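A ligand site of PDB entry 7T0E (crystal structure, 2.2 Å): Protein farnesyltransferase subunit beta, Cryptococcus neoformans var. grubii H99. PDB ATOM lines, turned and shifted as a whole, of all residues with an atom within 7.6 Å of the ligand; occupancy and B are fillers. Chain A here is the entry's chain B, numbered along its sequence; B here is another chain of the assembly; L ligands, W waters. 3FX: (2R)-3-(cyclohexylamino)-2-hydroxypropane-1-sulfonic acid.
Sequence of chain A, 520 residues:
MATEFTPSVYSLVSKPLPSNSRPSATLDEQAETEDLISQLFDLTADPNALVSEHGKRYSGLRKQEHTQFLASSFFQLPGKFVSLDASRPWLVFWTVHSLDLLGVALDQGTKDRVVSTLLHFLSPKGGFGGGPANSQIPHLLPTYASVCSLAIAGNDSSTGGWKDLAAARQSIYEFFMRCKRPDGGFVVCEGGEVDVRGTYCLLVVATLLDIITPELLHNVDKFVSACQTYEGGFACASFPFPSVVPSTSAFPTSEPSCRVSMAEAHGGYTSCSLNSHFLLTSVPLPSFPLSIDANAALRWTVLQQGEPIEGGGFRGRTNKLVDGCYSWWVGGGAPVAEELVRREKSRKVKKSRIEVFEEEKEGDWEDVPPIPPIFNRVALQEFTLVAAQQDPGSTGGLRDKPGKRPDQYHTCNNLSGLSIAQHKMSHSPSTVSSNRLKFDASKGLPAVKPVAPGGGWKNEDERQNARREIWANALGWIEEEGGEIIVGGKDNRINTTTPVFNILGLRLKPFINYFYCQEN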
ATOM      1  N   LEU A 122     -19.064  23.858 -17.795  1.00  0.00           N
ATOM      2  CA  LEU A 122     -19.876  24.839 -17.088  1.00  0.00           C
ATOM      3  C   LEU A 122     -20.035  26.091 -17.946  1.00  0.00           C
ATOM      4  O   LEU A 122     -19.044  26.691 -18.374  1.00  0.00           O
ATOM      5  CB  LEU A 122     -19.225  25.197 -15.751  1.00  0.00           C
ATOM      6  CG  LEU A 122     -19.953  26.239 -14.891  1.00  0.00           C
ATOM      7  CD1 LEU A 122     -21.374  25.798 -14.602  1.00  0.00           C
ATOM      8  CD2 LEU A 122     -19.179  26.478 -13.598  1.00  0.00           C
ATOM      9  N   SER A 123     -21.281  26.468 -18.187  1.00  0.00           N
ATOM     10  CA  SER A 123     -21.544  27.643 -19.023  1.00  0.00           C
ATOM     11  C   SER A 123     -21.648  28.899 -18.150  1.00  0.00           C
ATOM     12  O   SER A 123     -22.238  28.858 -17.071  1.00  0.00           O
ATOM     13  CB  SER A 123     -22.833  27.470 -19.812  1.00  0.00           C
ATOM     14  OG  SER A 123     -23.066  28.578 -20.663  1.00  0.00           O
ATOM     15  N   PRO A 124     -21.078  30.013 -18.611  1.00  0.00           N
ATOM     16  CA  PRO A 124     -21.174  31.259 -17.823  1.00  0.00           C
ATOM     17  C   PRO A 124     -22.595  31.719 -17.587  1.00  0.00           C
ATOM     18  O   PRO A 124     -22.865  32.397 -16.591  1.00  0.00           O
ATOM     19  CB  PRO A 124     -20.383  32.268 -18.663  1.00  0.00           C
ATOM     20  CG  PRO A 124     -19.457  31.432 -19.491  1.00  0.00           C
ATOM     21  CD  PRO A 124     -20.221  30.173 -19.799  1.00  0.00           C
ATOM     22  N   LYS A 125     -23.530  31.375 -18.476  1.00  0.00           N
ATOM     23  CA  LYS A 125     -24.926  31.755 -18.299  1.00  0.00           C
ATOM     24  C   LYS A 125     -25.651  30.876 -17.291  1.00  0.00           C
ATOM     25  O   LYS A 125     -26.771  31.225 -16.892  1.00  0.00           O
ATOM     26  CB  LYS A 125     -25.660  31.729 -19.642  1.00  0.00           C
ATOM     27  CG  LYS A 125     -25.630  30.402 -20.370  1.00  0.00           C
ATOM     28  CD  LYS A 125     -26.080  30.542 -21.819  1.00  0.00           C
ATOM     29  CE  LYS A 125     -25.874  29.264 -22.610  1.00  0.00           C
ATOM     30  NZ  LYS A 125     -26.206  29.428 -24.057  1.00  0.00           N
ATOM     31  N   GLY A 126     -25.064  29.767 -16.873  1.00  0.00           N
ATOM     32  CA  GLY A 126     -25.644  28.957 -15.815  1.00  0.00           C
ATOM     33  C   GLY A 126     -25.879  27.501 -16.165  1.00  0.00           C
ATOM     34  O   GLY A 126     -26.577  27.196 -17.123  1.00  0.00           O
ATOM     35  N   PRO A 132     -18.375  20.215 -23.596  1.00  0.00           N
ATOM     36  CA  PRO A 132     -17.794  21.566 -23.546  1.00  0.00           C
ATOM     37  C   PRO A 132     -18.844  22.652 -23.763  1.00  0.00           C
ATOM     38  O   PRO A 132     -19.743  22.522 -24.607  1.00  0.00           O
ATOM     39  CB  PRO A 132     -16.760  21.550 -24.675  1.00  0.00           C
ATOM     40  CG  PRO A 132     -16.340  20.127 -24.743  1.00  0.00           C
ATOM     41  CD  PRO A 132     -17.552  19.295 -24.410  1.00  0.00           C
ATOM     42  N   ALA A 133     -18.731  23.733 -22.987  1.00  0.00           N
ATOM     43  CA  ALA A 133     -19.692  24.826 -23.056  1.00  0.00           C
ATOM     44  C   ALA A 133     -19.674  25.526 -24.401  1.00  0.00           C
ATOM     45  O   ALA A 133     -20.658  26.188 -24.753  1.00  0.00           O
ATOM     46  CB  ALA A 133     -19.414  25.835 -21.935  1.00  0.00           C
ATOM     47  N   ASN A 134     -18.592  25.410 -25.170  1.00  0.00           N
ATOM     48  CA  ASN A 134     -18.561  25.970 -26.508  1.00  0.00           C
ATOM     49  C   ASN A 134     -19.237  25.072 -27.536  1.00  0.00           C
ATOM     50  O   ASN A 134     -19.205  25.382 -28.729  1.00  0.00           O
ATOM     51  CB  ASN A 134     -17.116  26.271 -26.939  1.00  0.00           C
ATOM     52  CG  ASN A 134     -16.399  25.039 -27.504  1.00  0.00           C
ATOM     53  OD1 ASN A 134     -16.618  23.921 -27.064  1.00  0.00           O
ATOM     54  ND2 ASN A 134     -15.533  25.272 -28.484  1.00  0.00           N
ATOM     55  N   SER A 135     -19.845  23.964 -27.089  1.00  0.00           N
ATOM     56  CA  SER A 135     -20.430  23.006 -28.018  1.00  0.00           C
ATOM     57  C   SER A 135     -21.836  22.576 -27.598  1.00  0.00           C
ATOM     58  O   SER A 135     -22.650  22.189 -28.451  1.00  0.00           O
ATOM     59  CB  SER A 135     -19.533  21.769 -28.132  1.00  0.00           C
ATOM     60  OG  SER A 135     -18.192  22.122 -28.427  1.00  0.00           O
ATOM     61  N   GLN A 136     -22.142  22.644 -26.300  1.00  0.00           N
ATOM     62  CA  GLN A 136     -23.412  22.144 -25.802  1.00  0.00           C
ATOM     63  C   GLN A 136     -24.016  23.140 -24.808  1.00  0.00           C
ATOM     64  O   GLN A 136     -23.288  23.776 -24.035  1.00  0.00           O
ATOM     65  CB  GLN A 136     -23.249  20.776 -25.139  1.00  0.00           C
ATOM     66  CG  GLN A 136     -22.781  19.686 -26.089  1.00  0.00           C
ATOM     67  CD  GLN A 136     -22.786  18.312 -25.455  1.00  0.00           C
ATOM     68  OE1 GLN A 136     -21.818  17.549 -25.575  1.00  0.00           O
ATOM     69  NE2 GLN A 136     -23.867  17.978 -24.768  1.00  0.00           N
ATOM     70  N   ILE A 137     -25.339  23.240 -24.826  1.00  0.00           N
ATOM     71  CA  ILE A 137     -26.065  24.158 -23.950  1.00  0.00           C
ATOM     72  C   ILE A 137     -26.307  23.480 -22.602  1.00  0.00           C
ATOM     73  O   ILE A 137     -26.316  22.243 -22.531  1.00  0.00           O
ATOM     74  CB  ILE A 137     -27.395  24.602 -24.597  1.00  0.00           C
ATOM     75  CG1 ILE A 137     -28.314  23.415 -24.838  1.00  0.00           C
ATOM     76  CG2 ILE A 137     -27.127  25.354 -25.897  1.00  0.00           C
ATOM     77  CD1 ILE A 137     -29.631  23.775 -25.502  1.00  0.00           C
ATOM     78  N   PRO A 138     -26.506  24.236 -21.525  1.00  0.00           N
ATOM     79  CA  PRO A 138     -26.705  23.618 -20.210  1.00  0.00           C
ATOM     80  C   PRO A 138     -27.971  22.768 -20.159  1.00  0.00           C
ATOM     81  O   PRO A 138     -28.922  22.968 -20.917  1.00  0.00           O
ATOM     82  CB  PRO A 138     -26.784  24.814 -19.250  1.00  0.00           C
ATOM     83  CG  PRO A 138     -27.086  25.992 -20.124  1.00  0.00           C
ATOM     84  CD  PRO A 138     -26.413  25.710 -21.426  1.00  0.00           C
ATOM     85  N   ILE B  35     -14.577  25.835 -35.735  1.00  0.00           N
ATOM     86  CA  ILE B  35     -14.170  26.065 -34.357  1.00  0.00           C
ATOM     87  C   ILE B  35     -13.999  24.719 -33.672  1.00  0.00           C
ATOM     88  O   ILE B  35     -14.889  23.873 -33.725  1.00  0.00           O
ATOM     89  CB  ILE B  35     -15.193  26.934 -33.593  1.00  0.00           C
ATOM     90  CG1 ILE B  35     -15.335  28.306 -34.269  1.00  0.00           C
ATOM     91  CG2 ILE B  35     -14.788  27.090 -32.135  1.00  0.00           C
ATOM     92  CD1 ILE B  35     -16.293  29.232 -33.557  1.00  0.00           C
ATOM     93  N   MET B  57     -19.294  18.666 -36.349  1.00  0.00           N
ATOM     94  CA  MET B  57     -19.397  19.432 -35.112  1.00  0.00           C
ATOM     95  C   MET B  57     -18.476  20.646 -35.113  1.00  0.00           C
ATOM     96  O   MET B  57     -18.805  21.670 -34.499  1.00  0.00           O
ATOM     97  CB  MET B  57     -19.086  18.545 -33.899  1.00  0.00           C
ATOM     98  CG  MET B  57     -20.204  17.573 -33.529  1.00  0.00           C
ATOM     99  SD  MET B  57     -21.793  18.355 -33.223  1.00  0.00           S
ATOM    100  CE  MET B  57     -21.359  19.572 -31.973  1.00  0.00           C
ATOM    101  N   PHE B  60     -20.456  23.068 -37.023  1.00  0.00           N
ATOM    102  CA  PHE B  60     -21.642  23.422 -36.247  1.00  0.00           C
ATOM    103  C   PHE B  60     -21.285  24.408 -35.130  1.00  0.00           C
ATOM    104  O   PHE B  60     -22.075  25.319 -34.835  1.00  0.00           O
ATOM    105  CB  PHE B  60     -22.293  22.181 -35.646  1.00  0.00           C
ATOM    106  CG  PHE B  60     -23.420  22.496 -34.699  1.00  0.00           C
ATOM    107  CD1 PHE B  60     -24.681  22.793 -35.185  1.00  0.00           C
ATOM    108  CD2 PHE B  60     -23.210  22.518 -33.336  1.00  0.00           C
ATOM    109  CE1 PHE B  60     -25.719  23.096 -34.317  1.00  0.00           C
ATOM    110  CE2 PHE B  60     -24.242  22.824 -32.456  1.00  0.00           C
ATOM    111  CZ  PHE B  60     -25.501  23.114 -32.950  1.00  0.00           C
ATOM    112  N   ARG B  61     -20.123  24.227 -34.497  1.00  0.00           N
ATOM    113  CA  ARG B  61     -19.687  25.177 -33.481  1.00  0.00           C
ATOM    114  C   ARG B  61     -19.549  26.578 -34.072  1.00  0.00           C
ATOM    115  O   ARG B  61     -19.818  27.573 -33.392  1.00  0.00           O
ATOM    116  CB  ARG B  61     -18.363  24.727 -32.871  1.00  0.00           C
ATOM    117  CG  ARG B  61     -18.513  23.813 -31.659  1.00  0.00           C
ATOM    118  CD  ARG B  61     -17.151  23.346 -31.149  1.00  0.00           C
ATOM    119  NE  ARG B  61     -16.566  22.324 -32.000  1.00  0.00           N
ATOM    120  CZ  ARG B  61     -16.783  21.019 -31.868  1.00  0.00           C
ATOM    121  NH1 ARG B  61     -17.597  20.580 -30.909  1.00  0.00           N
ATOM    122  NH2 ARG B  61     -16.209  20.160 -32.692  1.00  0.00           N
ATOM    123  N   ALA B  62     -19.128  26.664 -35.337  1.00  0.00           N
ATOM    124  CA  ALA B  62     -19.013  27.975 -35.974  1.00  0.00           C
ATOM    125  C   ALA B  62     -20.390  28.515 -36.362  1.00  0.00           C
ATOM    126  O   ALA B  62     -20.667  29.700 -36.157  1.00  0.00           O
ATOM    127  CB  ALA B  62     -18.114  27.875 -37.204  1.00  0.00           C
ATOM    128  N   ILE B  63     -21.252  27.655 -36.903  1.00  0.00           N
ATOM    129  CA  ILE B  63     -22.608  28.082 -37.280  1.00  0.00           C
ATOM    130  C   ILE B  63     -23.343  28.630 -36.069  1.00  0.00           C
ATOM    131  O   ILE B  63     -23.963  29.702 -36.132  1.00  0.00           O
ATOM    132  CB  ILE B  63     -23.374  26.913 -37.931  1.00  0.00           C
ATOM    133  CG1 ILE B  63     -22.853  26.643 -39.343  1.00  0.00           C
ATOM    134  CG2 ILE B  63     -24.868  27.198 -37.947  1.00  0.00           C
ATOM    135  CD1 ILE B  63     -23.172  27.734 -40.333  1.00  0.00           C
ATOM    136  N   ALA B  64     -23.280  27.907 -34.947  1.00  0.00           N
ATOM    137  CA  ALA B  64     -23.949  28.369 -33.739  1.00  0.00           C
ATOM    138  C   ALA B  64     -23.268  29.608 -33.169  1.00  0.00           C
ATOM    139  O   ALA B  64     -23.939  30.429 -32.522  1.00  0.00           O
ATOM    140  CB  ALA B  64     -23.972  27.252 -32.700  1.00  0.00           C
ATOM    141  N   ALA B  65     -21.965  29.771 -33.381  1.00  0.00           N
ATOM    142  CA  ALA B  65     -21.264  30.949 -32.889  1.00  0.00           C
ATOM    143  C   ALA B  65     -21.734  32.202 -33.606  1.00  0.00           C
ATOM    144  O   ALA B  65     -22.007  33.237 -32.976  1.00  0.00           O
ATOM    145  CB  ALA B  65     -19.757  30.770 -33.035  1.00  0.00           C
ATOM    146  N   GLU B  67     -24.535  32.355 -35.080  1.00  0.00           N
ATOM    147  CA  GLU B  67     -25.996  32.317 -34.974  1.00  0.00           C
ATOM    148  C   GLU B  67     -26.645  32.295 -36.358  1.00  0.00           C
ATOM    149  O   GLU B  67     -27.681  32.944 -36.585  1.00  0.00           O
ATOM    150  CB  GLU B  67     -26.516  33.487 -34.134  1.00  0.00           C
ATOM    151  CG  GLU B  67     -26.031  33.467 -32.705  1.00  0.00           C
ATOM    152  CD  GLU B  67     -26.540  34.647 -31.900  1.00  0.00           C
ATOM    153  OE1 GLU B  67     -27.360  35.421 -32.443  1.00  0.00           O
ATOM    154  OE2 GLU B  67     -26.113  34.804 -30.738  1.00  0.00           O
ATOM    155  N   HIS B  87     -28.163  14.092 -29.407  1.00  0.00           N
ATOM    156  CA  HIS B  87     -27.483  15.380 -29.252  1.00  0.00           C
ATOM    157  C   HIS B  87     -28.539  16.469 -29.090  1.00  0.00           C
ATOM    158  O   HIS B  87     -29.040  17.035 -30.063  1.00  0.00           O
ATOM    159  CB  HIS B  87     -26.580  15.647 -30.446  1.00  0.00           C
ATOM    160  CG  HIS B  87     -25.359  16.452 -30.124  1.00  0.00           C
ATOM    161  ND1 HIS B  87     -25.383  17.509 -29.231  1.00  0.00           N
ATOM    162  CD2 HIS B  87     -24.082  16.345 -30.546  1.00  0.00           C
ATOM    163  CE1 HIS B  87     -24.167  18.018 -29.133  1.00  0.00           C
ATOM    164  NE2 HIS B  87     -23.359  17.337 -29.921  1.00  0.00           N
ATOM    165  N   THR B  89     -28.451  19.517 -27.963  1.00  0.00           N
ATOM    166  CA  THR B  89     -28.124  20.879 -28.398  1.00  0.00           C
ATOM    167  C   THR B  89     -28.426  21.063 -29.886  1.00  0.00           C
ATOM    168  O   THR B  89     -28.992  22.089 -30.292  1.00  0.00           O
ATOM    169  CB  THR B  89     -26.655  21.183 -28.117  1.00  0.00           C
ATOM    170  OG1 THR B  89     -26.411  21.105 -26.711  1.00  0.00           O
ATOM    171  CG2 THR B  89     -26.286  22.573 -28.609  1.00  0.00           C
ATOM    172  N   VAL B  90     -28.067  20.072 -30.702  1.00  0.00           N
ATOM    173  CA  VAL B  90     -28.323  20.167 -32.139  1.00  0.00           C
ATOM    174  C   VAL B  90     -29.814  20.096 -32.432  1.00  0.00           C
ATOM    175  O   VAL B  90     -30.307  20.749 -33.359  1.00  0.00           O
ATOM    176  CB  VAL B  90     -27.529  19.079 -32.889  1.00  0.00           C
ATOM    177  CG1 VAL B  90     -27.655  19.258 -34.390  1.00  0.00           C
ATOM    178  CG2 VAL B  90     -26.069  19.113 -32.459  1.00  0.00           C
ATOM    179  N   GLN B  92     -32.119  21.286 -30.443  1.00  0.00           N
ATOM    180  CA  GLN B  92     -32.645  22.602 -30.093  1.00  0.00           C
ATOM    181  C   GLN B  92     -32.357  23.614 -31.202  1.00  0.00           C
ATOM    182  O   GLN B  92     -33.236  24.411 -31.559  1.00  0.00           O
ATOM    183  CB  GLN B  92     -32.047  23.083 -28.769  1.00  0.00           C
ATOM    184  CG  GLN B  92     -32.743  24.292 -28.150  1.00  0.00           C
ATOM    185  CD  GLN B  92     -32.336  25.605 -28.784  1.00  0.00           C
ATOM    186  OE1 GLN B  92     -31.207  25.766 -29.249  1.00  0.00           O
ATOM    187  NE2 GLN B  92     -33.269  26.558 -28.830  1.00  0.00           N
ATOM    188  N   TYR B  93     -31.152  23.583 -31.763  1.00  0.00           N
ATOM    189  CA  TYR B  93     -30.828  24.478 -32.868  1.00  0.00           C
ATOM    190  C   TYR B  93     -31.664  24.142 -34.099  1.00  0.00           C
ATOM    191  O   TYR B  93     -32.079  25.059 -34.826  1.00  0.00           O
ATOM    192  CB  TYR B  93     -29.341  24.419 -33.195  1.00  0.00           C
ATOM    193  CG  TYR B  93     -28.805  25.680 -33.837  1.00  0.00           C
ATOM    194  CD1 TYR B  93     -28.855  25.859 -35.214  1.00  0.00           C
ATOM    195  CD2 TYR B  93     -28.267  26.694 -33.065  1.00  0.00           C
ATOM    196  CE1 TYR B  93     -28.377  27.009 -35.809  1.00  0.00           C
ATOM    197  CE2 TYR B  93     -27.777  27.854 -33.652  1.00  0.00           C
ATOM    198  CZ  TYR B  93     -27.834  28.003 -35.017  1.00  0.00           C
ATOM    199  OH  TYR B  93     -27.355  29.150 -35.594  1.00  0.00           O
HETATM  200  OAA 3FX L   1     -21.098  32.649 -22.806  1.00  0.00           O
HETATM  201  OAB 3FX L   1     -23.434  32.518 -23.668  1.00  0.00           O
HETATM  202  OAC 3FX L   1     -22.898  31.072 -25.784  1.00  0.00           O
HETATM  203  OAD 3FX L   1     -22.694  31.581 -21.488  1.00  0.00           O
HETATM  204  CAE 3FX L   1     -23.360  25.851 -29.522  1.00  0.00           C
HETATM  205  CAF 3FX L   1     -22.110  26.740 -29.516  1.00  0.00           C
HETATM  206  CAG 3FX L   1     -23.750  25.365 -28.119  1.00  0.00           C
HETATM  207  CAH 3FX L   1     -22.208  27.873 -28.503  1.00  0.00           C
HETATM  208  CAI 3FX L   1     -23.813  26.501 -27.102  1.00  0.00           C
HETATM  209  CAJ 3FX L   1     -21.481  29.152 -25.964  1.00  0.00           C
HETATM  210  CAK 3FX L   1     -21.963  30.216 -23.762  1.00  0.00           C
HETATM  211  NAL 3FX L   1     -22.750  28.489 -26.207  1.00  0.00           N
HETATM  212  CAM 3FX L   1     -21.745  30.477 -25.254  1.00  0.00           C
HETATM  213  CAN 3FX L   1     -22.547  27.357 -27.104  1.00  0.00           C
HETATM  214  SAO 3FX L   1     -22.338  31.793 -22.936  1.00  0.00           S
HETATM  215  O   HOH W   1     -19.068  27.846 -30.356  1.00  0.00           O
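Pro 124 touches the ligand (CD to OAD, 3.3 Å).
Asn 134 touches the ligand (O to CAF, 3.3 Å).
O of Ser 135 touches CAG of the ligand, 3.4 Å away.
N of Gln 136 touches CAG of the ligand, at 3.6 Å.
Ile 137 touches the ligand (CG2 to CAI, 3.7 Å).
CB of Ala 64 of chain B touches CAE of the ligand, 3.5 Å away.
CG2 of Thr 89 of chain B touches CAG of the ligand, 3.8 Å away.
Of the 26 residues printed, 10 come within 4 Å of the ligand.
Water W1 lies within hydrogen-bond range of the backbone carbonyl oxygen of Asn 134 (3.0 Å) and the backbone carbonyl oxygen of Arg 61 of chain B (3.1 Å).
O of Ala 133 lies close to NAL of the ligand (3.4 Å).
The side-chain hydroxyl of Ser 123 lies within hydrogen-bond range of an oxygen (OAD) of the ligand (3.1 Å).
The backbone NH of Lys 125 is in hydrogen-bond range of an oxygen (OAD) of the ligand (3.1 Å).
N of Ile 137 sits at hydrogen-bond distance from OG1 of Thr 89 of chain B (3.0 Å).
The side-chain amide oxygen (OD1) of Asn 134 sits at hydrogen-bond distance from the side-chain hydroxyl (OG) of Ser 135 (2.8 Å).
OG of Ser 135 lies within hydrogen-bond range of NH1 of Arg 61 of chain B (3.0 Å).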
